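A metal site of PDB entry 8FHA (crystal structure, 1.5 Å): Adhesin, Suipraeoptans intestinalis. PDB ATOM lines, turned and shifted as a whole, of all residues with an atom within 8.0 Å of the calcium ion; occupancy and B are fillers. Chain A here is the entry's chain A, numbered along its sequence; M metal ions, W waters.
The backbone NH of Ala 124 is in hydrogen-bond range of the side-chain carboxylate of Glu 131, 2.8 Å away.
The backbone carbonyl oxygen (O) of Val 122 is in hydrogen-bond range of the backbone NH (N) of Glu 131 (2.9 Å).
The side-chain carboxylate of Glu 131 is in hydrogen-bond range of the side-chain hydroxyl of Ser 132, at 2.5 Å.
OD1 of Asp 123 sits close to N of Gly 126, at 3.0 Å.
OD2 of Asp 123 is in hydrogen-bond range of N of Lys 128 (2.7 Å).
The side-chain amide oxygen of Asn 7 lies within hydrogen-bond range of the backbone NH of Asp 123 (2.8 Å).
Five residues have an atom within 4 Å of the calcium ion: Asp 123, Asp 125, Asp 127, Lys 129 and Glu 131.
The nearest printed residue that does not touch the calcium ion is Gly 126 (4.5 Å).
The calcium ion is bound by OE2 of Glu 131 (2.3 Å), O of Lys 129 (2.4 Å), OD1 of Asp 127 (2.4 Å), OD1 of Asp 123 (2.4 Å), water W1 (2.4 Å) and OD1 of Asp 125 (2.4 Å).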
ATOM      1  N   ASN A   7     -18.540   8.192 -35.769  1.00  0.00           N
ATOM      2  CA  ASN A   7     -17.638   8.058 -34.597  1.00  0.00           C
ATOM      3  C   ASN A   7     -16.209   7.813 -35.067  1.00  0.00           C
ATOM      4  O   ASN A   7     -15.950   6.954 -35.906  1.00  0.00           O
ATOM      5  CB  ASN A   7     -18.110   6.965 -33.654  1.00  0.00           C
ATOM      6  CG  ASN A   7     -19.282   7.404 -32.813  1.00  0.00           C
ATOM      7  OD1 ASN A   7     -19.476   8.606 -32.608  1.00  0.00           O
ATOM      8  ND2 ASN A   7     -20.041   6.453 -32.300  1.00  0.00           N
ATOM      9  N   VAL A 122     -17.527  11.463 -29.422  1.00  0.00           N
ATOM     10  CA  VAL A 122     -18.158  10.143 -29.702  1.00  0.00           C
ATOM     11  C   VAL A 122     -19.645  10.200 -29.343  1.00  0.00           C
ATOM     12  O   VAL A 122     -19.999  10.648 -28.250  1.00  0.00           O
ATOM     13  CB  VAL A 122     -17.415   9.020 -28.958  1.00  0.00           C
ATOM     14  CG1 VAL A 122     -18.073   7.672 -29.200  1.00  0.00           C
ATOM     15  CG2 VAL A 122     -15.952   9.004 -29.371  1.00  0.00           C
ATOM     16  N   ASP A 123     -20.483   9.768 -30.285  1.00  0.00           N
ATOM     17  CA  ASP A 123     -21.939   9.563 -30.092  1.00  0.00           C
ATOM     18  C   ASP A 123     -22.154   8.104 -29.689  1.00  0.00           C
ATOM     19  O   ASP A 123     -22.275   7.265 -30.586  1.00  0.00           O
ATOM     20  CB  ASP A 123     -22.700   9.890 -31.383  1.00  0.00           C
ATOM     21  CG  ASP A 123     -24.188   9.603 -31.292  1.00  0.00           C
ATOM     22  OD1 ASP A 123     -24.700   9.592 -30.154  1.00  0.00           O
ATOM     23  OD2 ASP A 123     -24.794   9.359 -32.348  1.00  0.00           O
ATOM     24  N   ALA A 124     -22.145   7.815 -28.391  1.00  0.00           N
ATOM     25  CA  ALA A 124     -22.227   6.442 -27.860  1.00  0.00           C
ATOM     26  C   ALA A 124     -23.676   5.922 -27.876  1.00  0.00           C
ATOM     27  O   ALA A 124     -23.836   4.697 -27.978  1.00  0.00           O
ATOM     28  CB  ALA A 124     -21.634   6.388 -26.471  1.00  0.00           C
ATOM     29  N   ASP A 125     -24.698   6.798 -27.803  1.00  0.00           N
ATOM     30  CA  ASP A 125     -26.118   6.351 -27.697  1.00  0.00           C
ATOM     31  C   ASP A 125     -26.832   6.459 -29.055  1.00  0.00           C
ATOM     32  O   ASP A 125     -28.003   6.062 -29.132  1.00  0.00           O
ATOM     33  CB  ASP A 125     -26.863   7.051 -26.560  1.00  0.00           C
ATOM     34  CG  ASP A 125     -27.000   8.553 -26.719  1.00  0.00           C
ATOM     35  OD1 ASP A 125     -26.635   9.052 -27.785  1.00  0.00           O
ATOM     36  OD2 ASP A 125     -27.488   9.211 -25.766  1.00  0.00           O
ATOM     37  N   GLY A 126     -26.143   6.970 -30.090  1.00  0.00           N
ATOM     38  CA  GLY A 126     -26.598   6.915 -31.496  1.00  0.00           C
ATOM     39  C   GLY A 126     -27.747   7.860 -31.794  1.00  0.00           C
ATOM     40  O   GLY A 126     -28.579   7.512 -32.660  1.00  0.00           O
ATOM     41  N   ASP A 127     -27.814   9.018 -31.144  1.00  0.00           N
ATOM     42  CA  ASP A 127     -28.821  10.070 -31.445  1.00  0.00           C
ATOM     43  C   ASP A 127     -28.182  11.143 -32.340  1.00  0.00           C
ATOM     44  O   ASP A 127     -28.823  12.200 -32.540  1.00  0.00           O
ATOM     45  CB  ASP A 127     -29.416  10.664 -30.167  1.00  0.00           C
ATOM     46  CG  ASP A 127     -28.429  11.456 -29.337  1.00  0.00           C
ATOM     47  OD1 ASP A 127     -27.273  11.552 -29.774  1.00  0.00           O
ATOM     48  OD2 ASP A 127     -28.815  11.963 -28.276  1.00  0.00           O
ATOM     49  N   LYS A 128     -26.970  10.879 -32.847  1.00  0.00           N
ATOM     50  CA  LYS A 128     -26.250  11.713 -33.860  1.00  0.00           C
ATOM     51  C   LYS A 128     -25.657  12.967 -33.202  1.00  0.00           C
ATOM     52  O   LYS A 128     -25.319  13.909 -33.943  1.00  0.00           O
ATOM     53  CB  LYS A 128     -27.188  12.085 -35.015  1.00  0.00           C
ATOM     54  N   LYS A 129     -25.537  12.987 -31.872  1.00  0.00           N
ATOM     55  CA  LYS A 129     -24.974  14.114 -31.076  1.00  0.00           C
ATOM     56  C   LYS A 129     -23.851  13.580 -30.188  1.00  0.00           C
ATOM     57  O   LYS A 129     -24.106  12.765 -29.319  1.00  0.00           O
ATOM     58  CB  LYS A 129     -26.069  14.740 -30.195  1.00  0.00           C
ATOM     59  CG  LYS A 129     -27.054  15.669 -30.902  1.00  0.00           C
ATOM     60  CD  LYS A 129     -26.813  17.141 -30.606  1.00  0.00           C
ATOM     61  CE  LYS A 129     -27.433  18.090 -31.622  1.00  0.00           C
ATOM     62  NZ  LYS A 129     -28.883  18.275 -31.385  1.00  0.00           N
ATOM     63  N   PRO A 130     -22.579  13.978 -30.355  1.00  0.00           N
ATOM     64  CA  PRO A 130     -21.518  13.455 -29.492  1.00  0.00           C
ATOM     65  C   PRO A 130     -21.762  13.808 -28.007  1.00  0.00           C
ATOM     66  O   PRO A 130     -22.165  14.935 -27.715  1.00  0.00           O
ATOM     67  CB  PRO A 130     -20.239  14.107 -30.025  1.00  0.00           C
ATOM     68  CG  PRO A 130     -20.724  15.318 -30.790  1.00  0.00           C
ATOM     69  CD  PRO A 130     -22.078  14.934 -31.361  1.00  0.00           C
ATOM     70  N   GLU A 131     -21.527  12.851 -27.116  1.00  0.00           N
ATOM     71  CA  GLU A 131     -21.684  13.063 -25.649  1.00  0.00           C
ATOM     72  C   GLU A 131     -20.567  12.381 -24.859  1.00  0.00           C
ATOM     73  O   GLU A 131     -20.610  12.474 -23.638  1.00  0.00           O
ATOM     74  CB  GLU A 131     -23.060  12.582 -25.170  1.00  0.00           C
ATOM     75  CG  GLU A 131     -23.140  11.089 -24.880  1.00  0.00           C
ATOM     76  CD  GLU A 131     -22.928  10.221 -26.101  1.00  0.00           C
ATOM     77  OE1 GLU A 131     -21.924   9.500 -26.160  1.00  0.00           O
ATOM     78  OE2 GLU A 131     -23.739  10.290 -26.995  1.00  0.00           O
ATOM     79  N   SER A 132     -19.596  11.743 -25.523  1.00  0.00           N
ATOM     80  CA  SER A 132     -18.550  10.936 -24.854  1.00  0.00           C
ATOM     81  C   SER A 132     -17.174  11.347 -25.368  1.00  0.00           C
ATOM     82  O   SER A 132     -17.054  11.765 -26.545  1.00  0.00           O
ATOM     83  CB  SER A 132     -18.772   9.457 -25.057  1.00  0.00           C
ATOM     84  OG  SER A 132     -20.031   9.041 -24.568  1.00  0.00           O
HETATM   85 CA    CA M   1     -25.417  11.036 -28.377  1.00  0.00          CA
HETATM   86  O   HOH W   1     -26.308  12.651 -26.842  1.00  0.00           O
